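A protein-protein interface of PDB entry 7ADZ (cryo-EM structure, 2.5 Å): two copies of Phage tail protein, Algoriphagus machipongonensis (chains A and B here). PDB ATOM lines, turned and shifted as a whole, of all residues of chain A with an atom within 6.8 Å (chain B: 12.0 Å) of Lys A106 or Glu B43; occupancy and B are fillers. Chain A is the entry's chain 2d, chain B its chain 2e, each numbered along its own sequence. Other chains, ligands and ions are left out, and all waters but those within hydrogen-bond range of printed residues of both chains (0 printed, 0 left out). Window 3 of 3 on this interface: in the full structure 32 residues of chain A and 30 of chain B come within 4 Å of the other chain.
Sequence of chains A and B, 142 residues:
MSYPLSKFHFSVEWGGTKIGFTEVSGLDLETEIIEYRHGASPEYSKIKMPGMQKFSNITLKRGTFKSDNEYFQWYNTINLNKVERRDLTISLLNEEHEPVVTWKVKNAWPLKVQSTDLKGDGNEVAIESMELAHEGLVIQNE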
ATOM      1  N   MET A  52      27.762  29.787 -12.436  1.00  0.00           N
ATOM      2  CA  MET A  52      27.171  29.699 -13.771  1.00  0.00           C
ATOM      3  C   MET A  52      25.676  29.332 -13.750  1.00  0.00           C
ATOM      4  O   MET A  52      25.160  28.805 -12.760  1.00  0.00           O
ATOM      5  CB  MET A  52      27.967  28.719 -14.608  1.00  0.00           C
ATOM      6  CG  MET A  52      29.380  29.217 -14.910  1.00  0.00           C
ATOM      7  SD  MET A  52      30.384  28.086 -15.870  1.00  0.00           S
ATOM      8  CE  MET A  52      29.673  28.242 -17.497  1.00  0.00           C
ATOM      9  N   GLN A  53      24.978  29.649 -14.849  1.00  0.00           N
ATOM     10  CA  GLN A  53      23.528  29.428 -14.989  1.00  0.00           C
ATOM     11  C   GLN A  53      23.168  28.095 -15.655  1.00  0.00           C
ATOM     12  O   GLN A  53      23.906  27.609 -16.512  1.00  0.00           O
ATOM     13  CB  GLN A  53      22.949  30.500 -15.912  1.00  0.00           C
ATOM     14  CG  GLN A  53      23.234  31.954 -15.563  1.00  0.00           C
ATOM     15  CD  GLN A  53      22.626  32.486 -14.338  1.00  0.00           C
ATOM     16  OE1 GLN A  53      21.414  32.405 -14.151  1.00  0.00           O
ATOM     17  NE2 GLN A  53      23.454  33.076 -13.498  1.00  0.00           N
ATOM     18  N   ARG A  86      13.195  27.045 -32.946  1.00  0.00           N
ATOM     19  CA  ARG A  86      12.034  27.923 -32.850  1.00  0.00           C
ATOM     20  C   ARG A  86      11.901  28.719 -31.556  1.00  0.00           C
ATOM     21  O   ARG A  86      12.377  28.327 -30.489  1.00  0.00           O
ATOM     22  CB  ARG A  86      10.758  27.107 -33.010  1.00  0.00           C
ATOM     23  CG  ARG A  86      10.603  26.375 -34.334  1.00  0.00           C
ATOM     24  CD  ARG A  86       9.322  25.665 -34.412  1.00  0.00           C
ATOM     25  NE  ARG A  86       9.213  24.886 -35.612  1.00  0.00           N
ATOM     26  CZ  ARG A  86       8.225  24.036 -35.910  1.00  0.00           C
ATOM     27  NH1 ARG A  86       7.212  23.839 -35.102  1.00  0.00           N
ATOM     28  NH2 ARG A  86       8.298  23.403 -37.055  1.00  0.00           N
ATOM     29  N   ASP A  87      11.180  29.822 -31.650  1.00  0.00           N
ATOM     30  CA  ASP A  87      10.825  30.624 -30.488  1.00  0.00           C
ATOM     31  C   ASP A  87       9.533  30.098 -29.896  1.00  0.00           C
ATOM     32  O   ASP A  87       8.535  29.960 -30.600  1.00  0.00           O
ATOM     33  CB  ASP A  87      10.694  32.087 -30.852  1.00  0.00           C
ATOM     34  CG  ASP A  87      12.032  32.722 -31.182  1.00  0.00           C
ATOM     35  OD1 ASP A  87      13.056  32.241 -30.734  1.00  0.00           O
ATOM     36  OD2 ASP A  87      12.025  33.679 -31.901  1.00  0.00           O
ATOM     37  N   LEU A  88       9.586  29.715 -28.634  1.00  0.00           N
ATOM     38  CA  LEU A  88       8.456  29.128 -27.931  1.00  0.00           C
ATOM     39  C   LEU A  88       7.810  30.111 -26.949  1.00  0.00           C
ATOM     40  O   LEU A  88       8.466  30.635 -26.048  1.00  0.00           O
ATOM     41  CB  LEU A  88       8.966  27.852 -27.231  1.00  0.00           C
ATOM     42  CG  LEU A  88       8.034  27.073 -26.272  1.00  0.00           C
ATOM     43  CD1 LEU A  88       6.865  26.471 -27.017  1.00  0.00           C
ATOM     44  CD2 LEU A  88       8.852  25.997 -25.580  1.00  0.00           C
ATOM     45  N   LYS A 104       8.821  33.318 -22.001  1.00  0.00           N
ATOM     46  CA  LYS A 104       9.473  33.434 -23.301  1.00  0.00           C
ATOM     47  C   LYS A 104      10.708  32.553 -23.418  1.00  0.00           C
ATOM     48  O   LYS A 104      11.671  32.733 -22.671  1.00  0.00           O
ATOM     49  CB  LYS A 104       9.874  34.879 -23.508  1.00  0.00           C
ATOM     50  CG  LYS A 104       8.726  35.829 -23.573  1.00  0.00           C
ATOM     51  CD  LYS A 104       9.215  37.231 -23.720  1.00  0.00           C
ATOM     52  CE  LYS A 104       8.078  38.202 -23.833  1.00  0.00           C
ATOM     53  NZ  LYS A 104       8.568  39.595 -23.990  1.00  0.00           N
ATOM     54  N   VAL A 105      10.705  31.607 -24.363  1.00  0.00           N
ATOM     55  CA  VAL A 105      11.811  30.664 -24.519  1.00  0.00           C
ATOM     56  C   VAL A 105      12.546  30.764 -25.862  1.00  0.00           C
ATOM     57  O   VAL A 105      11.963  30.666 -26.945  1.00  0.00           O
ATOM     58  CB  VAL A 105      11.280  29.244 -24.286  1.00  0.00           C
ATOM     59  CG1 VAL A 105      12.363  28.222 -24.504  1.00  0.00           C
ATOM     60  CG2 VAL A 105      10.764  29.142 -22.882  1.00  0.00           C
ATOM     61  N   LYS A 106      13.857  30.935 -25.761  1.00  0.00           N
ATOM     62  CA  LYS A 106      14.788  31.095 -26.883  1.00  0.00           C
ATOM     63  C   LYS A 106      15.379  29.787 -27.464  1.00  0.00           C
ATOM     64  O   LYS A 106      15.881  28.949 -26.713  1.00  0.00           O
ATOM     65  CB  LYS A 106      15.915  31.985 -26.372  1.00  0.00           C
ATOM     66  CG  LYS A 106      16.974  32.378 -27.354  1.00  0.00           C
ATOM     67  CD  LYS A 106      17.910  33.442 -26.757  1.00  0.00           C
ATOM     68  CE  LYS A 106      18.792  32.860 -25.641  1.00  0.00           C
ATOM     69  NZ  LYS A 106      19.804  33.813 -25.166  1.00  0.00           N
ATOM     70  N   ASN A 107      15.421  29.669 -28.805  1.00  0.00           N
ATOM     71  CA  ASN A 107      16.040  28.537 -29.536  1.00  0.00           C
ATOM     72  C   ASN A 107      15.608  27.094 -29.195  1.00  0.00           C
ATOM     73  O   ASN A 107      16.461  26.225 -29.013  1.00  0.00           O
ATOM     74  CB  ASN A 107      17.559  28.617 -29.453  1.00  0.00           C
ATOM     75  CG  ASN A 107      18.140  29.770 -30.208  1.00  0.00           C
ATOM     76  OD1 ASN A 107      17.544  30.231 -31.184  1.00  0.00           O
ATOM     77  ND2 ASN A 107      19.292  30.234 -29.822  1.00  0.00           N
ATOM     78  N   ALA A 108      14.348  26.791 -29.022  1.00  0.00           N
ATOM     79  CA  ALA A 108      14.020  25.419 -28.713  1.00  0.00           C
ATOM     80  C   ALA A 108      14.171  24.417 -29.880  1.00  0.00           C
ATOM     81  O   ALA A 108      14.083  24.775 -31.034  1.00  0.00           O
ATOM     82  CB  ALA A 108      12.642  25.357 -28.100  1.00  0.00           C
ATOM     83  N   TRP A 109      14.511  23.179 -29.548  1.00  0.00           N
ATOM     84  CA  TRP A 109      14.559  22.057 -30.488  1.00  0.00           C
ATOM     85  C   TRP A 109      14.298  20.746 -29.727  1.00  0.00           C
ATOM     86  O   TRP A 109      14.743  20.578 -28.624  1.00  0.00           O
ATOM     87  CB  TRP A 109      15.836  22.026 -31.383  1.00  0.00           C
ATOM     88  CG  TRP A 109      17.145  21.986 -30.675  1.00  0.00           C
ATOM     89  CD1 TRP A 109      17.846  23.039 -30.222  1.00  0.00           C
ATOM     90  CD2 TRP A 109      17.903  20.825 -30.335  1.00  0.00           C
ATOM     91  NE1 TRP A 109      18.989  22.625 -29.626  1.00  0.00           N
ATOM     92  CE2 TRP A 109      19.052  21.264 -29.669  1.00  0.00           C
ATOM     93  CE3 TRP A 109      17.717  19.455 -30.522  1.00  0.00           C
ATOM     94  CZ2 TRP A 109      20.019  20.394 -29.199  1.00  0.00           C
ATOM     95  CZ3 TRP A 109      18.665  18.598 -30.049  1.00  0.00           C
ATOM     96  CH2 TRP A 109      19.805  19.068 -29.392  1.00  0.00           C
ATOM     97  N   ALA A 133      14.856  21.065 -25.708  1.00  0.00           N
ATOM     98  CA  ALA A 133      16.063  21.739 -25.253  1.00  0.00           C
ATOM     99  C   ALA A 133      15.912  23.207 -25.591  1.00  0.00           C
ATOM    100  O   ALA A 133      15.238  23.531 -26.565  1.00  0.00           O
ATOM    101  CB  ALA A 133      17.290  21.165 -25.920  1.00  0.00           C
ATOM    102  N   HIS A 134      16.529  24.102 -24.832  1.00  0.00           N
ATOM    103  CA  HIS A 134      16.461  25.526 -25.173  1.00  0.00           C
ATOM    104  C   HIS A 134      17.644  26.269 -24.584  1.00  0.00           C
ATOM    105  O   HIS A 134      18.448  25.685 -23.860  1.00  0.00           O
ATOM    106  CB  HIS A 134      15.143  26.125 -24.709  1.00  0.00           C
ATOM    107  CG  HIS A 134      14.980  26.151 -23.271  1.00  0.00           C
ATOM    108  ND1 HIS A 134      15.334  27.232 -22.490  1.00  0.00           N
ATOM    109  CD2 HIS A 134      14.546  25.207 -22.440  1.00  0.00           C
ATOM    110  CE1 HIS A 134      15.095  26.936 -21.238  1.00  0.00           C
ATOM    111  NE2 HIS A 134      14.629  25.700 -21.187  1.00  0.00           N
ATOM    112  N   GLU A 135      17.775  27.546 -24.925  1.00  0.00           N
ATOM    113  CA  GLU A 135      18.885  28.369 -24.452  1.00  0.00           C
ATOM    114  C   GLU A 135      18.522  29.566 -23.576  1.00  0.00           C
ATOM    115  O   GLU A 135      19.300  30.518 -23.493  1.00  0.00           O
ATOM    116  CB  GLU A 135      19.723  28.837 -25.641  1.00  0.00           C
ATOM    117  CG  GLU A 135      20.418  27.703 -26.386  1.00  0.00           C
ATOM    118  CD  GLU A 135      21.280  28.157 -27.522  1.00  0.00           C
ATOM    119  OE1 GLU A 135      21.241  29.315 -27.842  1.00  0.00           O
ATOM    120  OE2 GLU A 135      21.972  27.346 -28.077  1.00  0.00           O
ATOM    121  N   GLY A 136      17.366  29.566 -22.925  1.00  0.00           N
ATOM    122  CA  GLY A 136      17.057  30.699 -22.068  1.00  0.00           C
ATOM    123  C   GLY A 136      15.586  30.992 -21.898  1.00  0.00           C
ATOM    124  O   GLY A 136      14.785  30.866 -22.824  1.00  0.00           O
ATOM    125  N   LEU A 137      15.256  31.466 -20.696  1.00  0.00           N
ATOM    126  CA  LEU A 137      13.901  31.785 -20.274  1.00  0.00           C
ATOM    127  C   LEU A 137      13.756  33.139 -19.583  1.00  0.00           C
ATOM    128  O   LEU A 137      14.460  33.439 -18.621  1.00  0.00           O
ATOM    129  CB  LEU A 137      13.400  30.666 -19.339  1.00  0.00           C
ATOM    130  CG  LEU A 137      12.050  30.886 -18.600  1.00  0.00           C
ATOM    131  CD1 LEU A 137      10.905  30.973 -19.576  1.00  0.00           C
ATOM    132  CD2 LEU A 137      11.814  29.721 -17.627  1.00  0.00           C
ATOM    133  N   VAL A 138      12.800  33.926 -20.065  1.00  0.00           N
ATOM    134  CA  VAL A 138      12.435  35.227 -19.505  1.00  0.00           C
ATOM    135  C   VAL A 138      10.968  35.231 -19.072  1.00  0.00           C
ATOM    136  O   VAL A 138      10.089  34.787 -19.809  1.00  0.00           O
ATOM    137  CB  VAL A 138      12.705  36.354 -20.516  1.00  0.00           C
ATOM    138  CG1 VAL A 138      12.260  37.703 -19.967  1.00  0.00           C
ATOM    139  CG2 VAL A 138      14.180  36.389 -20.822  1.00  0.00           C
ATOM    140  N   ILE B  33      22.804  15.398 -26.775  1.00  0.00           N
ATOM    141  CA  ILE B  33      23.087  16.834 -26.830  1.00  0.00           C
ATOM    142  C   ILE B  33      24.564  17.152 -26.640  1.00  0.00           C
ATOM    143  O   ILE B  33      25.189  16.680 -25.694  1.00  0.00           O
ATOM    144  CB  ILE B  33      22.300  17.614 -25.749  1.00  0.00           C
ATOM    145  CG1 ILE B  33      20.811  17.425 -25.982  1.00  0.00           C
ATOM    146  CG2 ILE B  33      22.689  19.130 -25.773  1.00  0.00           C
ATOM    147  CD1 ILE B  33      19.933  17.928 -24.867  1.00  0.00           C
ATOM    148  N   GLU B  35      27.186  20.136 -25.833  1.00  0.00           N
ATOM    149  CA  GLU B  35      27.229  21.475 -25.227  1.00  0.00           C
ATOM    150  C   GLU B  35      28.562  22.213 -25.428  1.00  0.00           C
ATOM    151  O   GLU B  35      29.621  21.587 -25.430  1.00  0.00           O
ATOM    152  CB  GLU B  35      26.970  21.355 -23.736  1.00  0.00           C
ATOM    153  CG  GLU B  35      25.626  20.814 -23.350  1.00  0.00           C
ATOM    154  CD  GLU B  35      25.479  20.722 -21.866  1.00  0.00           C
ATOM    155  OE1 GLU B  35      26.493  20.773 -21.201  1.00  0.00           O
ATOM    156  OE2 GLU B  35      24.381  20.558 -21.389  1.00  0.00           O
ATOM    157  N   TYR B  36      28.516  23.551 -25.511  1.00  0.00           N
ATOM    158  CA  TYR B  36      29.746  24.349 -25.646  1.00  0.00           C
ATOM    159  C   TYR B  36      29.710  25.792 -25.094  1.00  0.00           C
ATOM    160  O   TYR B  36      28.699  26.484 -25.181  1.00  0.00           O
ATOM    161  CB  TYR B  36      30.098  24.421 -27.134  1.00  0.00           C
ATOM    162  CG  TYR B  36      31.366  25.136 -27.480  1.00  0.00           C
ATOM    163  CD1 TYR B  36      32.550  24.467 -27.445  1.00  0.00           C
ATOM    164  CD2 TYR B  36      31.342  26.465 -27.833  1.00  0.00           C
ATOM    165  CE1 TYR B  36      33.706  25.111 -27.765  1.00  0.00           C
ATOM    166  CE2 TYR B  36      32.496  27.109 -28.151  1.00  0.00           C
ATOM    167  CZ  TYR B  36      33.676  26.434 -28.122  1.00  0.00           C
ATOM    168  OH  TYR B  36      34.840  27.069 -28.446  1.00  0.00           O
ATOM    169  N   ARG B  37      30.819  26.250 -24.508  1.00  0.00           N
ATOM    170  CA  ARG B  37      30.973  27.655 -24.107  1.00  0.00           C
ATOM    171  C   ARG B  37      32.429  28.091 -24.193  1.00  0.00           C
ATOM    172  O   ARG B  37      33.312  27.359 -23.756  1.00  0.00           O
ATOM    173  CB  ARG B  37      30.470  27.948 -22.686  1.00  0.00           C
ATOM    174  CG  ARG B  37      30.645  29.437 -22.270  1.00  0.00           C
ATOM    175  CD  ARG B  37      30.101  29.847 -20.944  1.00  0.00           C
ATOM    176  NE  ARG B  37      30.366  31.297 -20.743  1.00  0.00           N
ATOM    177  CZ  ARG B  37      31.512  31.830 -20.211  1.00  0.00           C
ATOM    178  NH1 ARG B  37      32.472  31.044 -19.775  1.00  0.00           N
ATOM    179  NH2 ARG B  37      31.703  33.142 -20.129  1.00  0.00           N
ATOM    180  N   HIS B  38      32.687  29.304 -24.676  1.00  0.00           N
ATOM    181  CA  HIS B  38      34.047  29.820 -24.654  1.00  0.00           C
ATOM    182  C   HIS B  38      34.119  30.939 -23.609  1.00  0.00           C
ATOM    183  O   HIS B  38      33.112  31.569 -23.280  1.00  0.00           O
ATOM    184  CB  HIS B  38      34.492  30.292 -26.039  1.00  0.00           C
ATOM    185  CG  HIS B  38      33.772  31.468 -26.571  1.00  0.00           C
ATOM    186  ND1 HIS B  38      32.575  31.373 -27.214  1.00  0.00           N
ATOM    187  CD2 HIS B  38      34.096  32.765 -26.575  1.00  0.00           C
ATOM    188  CE1 HIS B  38      32.192  32.574 -27.585  1.00  0.00           C
ATOM    189  NE2 HIS B  38      33.100  33.433 -27.207  1.00  0.00           N
ATOM    190  N   GLY B  39      35.318  31.200 -23.106  1.00  0.00           N
ATOM    191  CA  GLY B  39      35.538  32.149 -22.015  1.00  0.00           C
ATOM    192  C   GLY B  39      35.061  33.584 -22.173  1.00  0.00           C
ATOM    193  O   GLY B  39      34.675  34.205 -21.185  1.00  0.00           O
ATOM    194  N   ALA B  40      35.079  34.120 -23.376  1.00  0.00           N
ATOM    195  CA  ALA B  40      34.672  35.499 -23.584  1.00  0.00           C
ATOM    196  C   ALA B  40      33.173  35.718 -23.736  1.00  0.00           C
ATOM    197  O   ALA B  40      32.755  36.856 -23.927  1.00  0.00           O
ATOM    198  CB  ALA B  40      35.363  36.052 -24.809  1.00  0.00           C
ATOM    199  N   SER B  41      32.356  34.673 -23.731  1.00  0.00           N
ATOM    200  CA  SER B  41      30.935  34.906 -23.933  1.00  0.00           C
ATOM    201  C   SER B  41      30.295  35.733 -22.798  1.00  0.00           C
ATOM    202  O   SER B  41      30.536  35.448 -21.625  1.00  0.00           O
ATOM    203  CB  SER B  41      30.190  33.608 -24.031  1.00  0.00           C
ATOM    204  OG  SER B  41      28.805  33.853 -24.124  1.00  0.00           O
ATOM    205  N   PRO B  42      29.458  36.757 -23.099  1.00  0.00           N
ATOM    206  CA  PRO B  42      28.661  37.541 -22.164  1.00  0.00           C
ATOM    207  C   PRO B  42      27.635  36.723 -21.379  1.00  0.00           C
ATOM    208  O   PRO B  42      27.101  37.196 -20.382  1.00  0.00           O
ATOM    209  CB  PRO B  42      27.941  38.526 -23.076  1.00  0.00           C
ATOM    210  CG  PRO B  42      28.787  38.629 -24.275  1.00  0.00           C
ATOM    211  CD  PRO B  42      29.394  37.272 -24.466  1.00  0.00           C
ATOM    212  N   GLU B  43      27.286  35.538 -21.872  1.00  0.00           N
ATOM    213  CA  GLU B  43      26.330  34.704 -21.170  1.00  0.00           C
ATOM    214  C   GLU B  43      27.090  33.622 -20.460  1.00  0.00           C
ATOM    215  O   GLU B  43      28.091  33.122 -20.975  1.00  0.00           O
ATOM    216  CB  GLU B  43      25.288  34.098 -22.099  1.00  0.00           C
ATOM    217  CG  GLU B  43      24.363  35.088 -22.735  1.00  0.00           C
ATOM    218  CD  GLU B  43      23.288  34.424 -23.560  1.00  0.00           C
ATOM    219  OE1 GLU B  43      23.362  33.234 -23.731  1.00  0.00           O
ATOM    220  OE2 GLU B  43      22.394  35.100 -24.006  1.00  0.00           O
ATOM    221  N   TYR B  44      26.567  33.182 -19.327  1.00  0.00           N
ATOM    222  CA  TYR B  44      27.264  32.182 -18.549  1.00  0.00           C
ATOM    223  C   TYR B  44      26.643  30.796 -18.664  1.00  0.00           C
ATOM    224  O   TYR B  44      26.887  29.916 -17.844  1.00  0.00           O
ATOM    225  CB  TYR B  44      27.362  32.697 -17.127  1.00  0.00           C
ATOM    226  CG  TYR B  44      27.975  34.105 -17.133  1.00  0.00           C
ATOM    227  CD1 TYR B  44      27.249  35.167 -16.654  1.00  0.00           C
ATOM    228  CD2 TYR B  44      29.213  34.339 -17.691  1.00  0.00           C
ATOM    229  CE1 TYR B  44      27.757  36.437 -16.717  1.00  0.00           C
ATOM    230  CE2 TYR B  44      29.713  35.613 -17.761  1.00  0.00           C
ATOM    231  CZ  TYR B  44      28.986  36.658 -17.274  1.00  0.00           C
ATOM    232  OH  TYR B  44      29.478  37.934 -17.338  1.00  0.00           O
ATOM    233  N   SER B  45      25.850  30.620 -19.707  1.00  0.00           N
ATOM    234  CA  SER B  45      25.195  29.375 -20.062  1.00  0.00           C
ATOM    235  C   SER B  45      25.850  28.794 -21.310  1.00  0.00           C
ATOM    236  O   SER B  45      26.607  29.473 -21.999  1.00  0.00           O
ATOM    237  CB  SER B  45      23.727  29.604 -20.324  1.00  0.00           C
ATOM    238  OG  SER B  45      23.059  30.040 -19.180  1.00  0.00           O
ATOM    239  N   LYS B  46      25.564  27.534 -21.610  1.00  0.00           N
ATOM    240  CA  LYS B  46      26.127  26.872 -22.788  1.00  0.00           C
ATOM    241  C   LYS B  46      25.196  26.865 -23.996  1.00  0.00           C
ATOM    242  O   LYS B  46      23.976  26.923 -23.851  1.00  0.00           O
ATOM    243  CB  LYS B  46      26.495  25.452 -22.417  1.00  0.00           C
ATOM    244  CG  LYS B  46      27.574  25.379 -21.371  1.00  0.00           C
ATOM    245  CD  LYS B  46      27.875  23.979 -21.011  1.00  0.00           C
ATOM    246  CE  LYS B  46      28.918  23.881 -19.942  1.00  0.00           C
ATOM    247  NZ  LYS B  46      29.124  22.474 -19.523  1.00  0.00           N
ATOM    248  N   ILE B  47      25.778  26.726 -25.188  1.00  0.00           N
ATOM    249  CA  ILE B  47      25.012  26.591 -26.427  1.00  0.00           C
ATOM    250  C   ILE B  47      24.872  25.112 -26.749  1.00  0.00           C
ATOM    251  O   ILE B  47      25.779  24.320 -26.494  1.00  0.00           O
ATOM    252  CB  ILE B  47      25.618  27.377 -27.610  1.00  0.00           C
ATOM    253  CG1 ILE B  47      27.037  26.879 -27.954  1.00  0.00           C
ATOM    254  CG2 ILE B  47      25.624  28.848 -27.237  1.00  0.00           C
ATOM    255  CD1 ILE B  47      27.613  27.397 -29.231  1.00  0.00           C
ATOM    256  N   LYS B  48      23.702  24.709 -27.240  1.00  0.00           N
ATOM    257  CA  LYS B  48      23.449  23.291 -27.495  1.00  0.00           C
ATOM    258  C   LYS B  48      23.199  22.921 -28.957  1.00  0.00           C
ATOM    259  O   LYS B  48      22.490  23.632 -29.664  1.00  0.00           O
ATOM    260  CB  LYS B  48      22.221  22.939 -26.676  1.00  0.00           C
ATOM    261  CG  LYS B  48      22.435  23.170 -25.208  1.00  0.00           C
ATOM    262  CD  LYS B  48      21.221  22.915 -24.401  1.00  0.00           C
ATOM    263  CE  LYS B  48      21.492  23.253 -22.959  1.00  0.00           C
ATOM    264  NZ  LYS B  48      20.309  23.041 -22.104  1.00  0.00           N
ATOM    265  N   MET B  49      23.708  21.759 -29.378  1.00  0.00           N
ATOM    266  CA  MET B  49      23.424  21.243 -30.721  1.00  0.00           C
ATOM    267  C   MET B  49      23.220  19.712 -30.699  1.00  0.00           C
ATOM    268  O   MET B  49      23.750  19.042 -29.819  1.00  0.00           O
ATOM    269  CB  MET B  49      24.544  21.609 -31.688  1.00  0.00           C
ATOM    270  CG  MET B  49      25.865  20.983 -31.396  1.00  0.00           C
ATOM    271  SD  MET B  49      27.117  21.509 -32.538  1.00  0.00           S
ATOM    272  CE  MET B  49      28.464  20.481 -32.047  1.00  0.00           C
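Of the 17 printed residues of chain A, 6 touch a printed residue of chain B. Printed residues of chain B that touch a printed residue of chain A: Ile B33, Arg B37, Glu B43, Tyr B44, Ser B45, Ile B47, Lys B48 and Met B49. Hydrophobic or aromatic side chains of chain B within 4 Å of the printed part of chain A: Ile B33 and Ile B47. Among the printed residues, Asp or Glu carboxylates within 4 Å of a Lys or Arg side-chain nitrogen of the other chain: Lys A106 with Glu B43.
NZ of Lys A106 is in salt-bridge range of OE2 of Glu B43, 3.1 Å away. The backbone NH (N) of Lys B48 sits at hydrogen-bond distance from the side-chain carboxylate (OE2) of Glu A135 (3.3 Å).
Among the printed residues, merely in contact across the chains: Met A52 with Arg B37 (3.8 Å), Met A52 with Tyr B44 (3.3 Å), Gln A53 with Tyr B44 (3.6 Å), Gln A53 with Ser B45 (3.3 Å), Trp A109 with Ile B33 (3.9 Å), Trp A109 with Lys B48 (3.6 Å), Trp A109 with Met B49 (3.6 Å), His A134 with Lys B48 (3.7 Å) and Glu A135 with Ile B47 (3.5 Å).
The backbone NH (N) of Glu A135 sits at hydrogen-bond distance from the backbone carbonyl oxygen (O) of Lys A106 (3.0 Å). ND2 of Asn A107 lies within hydrogen-bond range of OE1 of Glu A135, 2.9 Å away. The backbone carbonyl oxygen (O) of Trp A109 sits at hydrogen-bond distance from the backbone NH (N) of Ala A133 (3.0 Å). The guanidinium group (NH2) of Arg B37 is in hydrogen-bond range of the backbone carbonyl oxygen (O) of Gly B39. The backbone carbonyl oxygen (O) of Ser B41 sits at hydrogen-bond distance from the guanidinium group (NH2) of Arg B37, 3.0 Å away. The guanidinium group of Arg B37 is in hydrogen-bond range of the backbone carbonyl oxygen of Glu B43, 2.9 Å away.
Of the printed residues of chain B, Met A52 touches Arg B37 and Tyr B44. Of the printed residues of chain B, Gln A53 touches Tyr B44 and Ser B45. No residue of chain B comes within 4 Å of Asp A87. Lys A106 touches just one residue of chain B: Glu B43. No residue of chain B comes within 4 Å of Asn A107. No residue of chain B comes within 4 Å of Ala A108. Of the printed residues of chain B, His A134 touches Lys B48 (3.7 Å). No residue of chain B comes within 4 Å of Gly A136. His B38 touches none of the printed residues of chain A. Of the printed residues of chain A, Tyr B44 touches Met A52 (3.3 Å) and Gln A53 (3.6 Å). The nearest residue of chain B that does not touch Lys A106 is Ser B45 (7.5 Å). The nearest residue of chain A that does not touch Glu B43 is Glu A135 (4.9 Å).
No position is printed for both chains. Of the 11 pairs that touch across the chains among the printed residues, none has its exchanged pair printed and touching as well.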
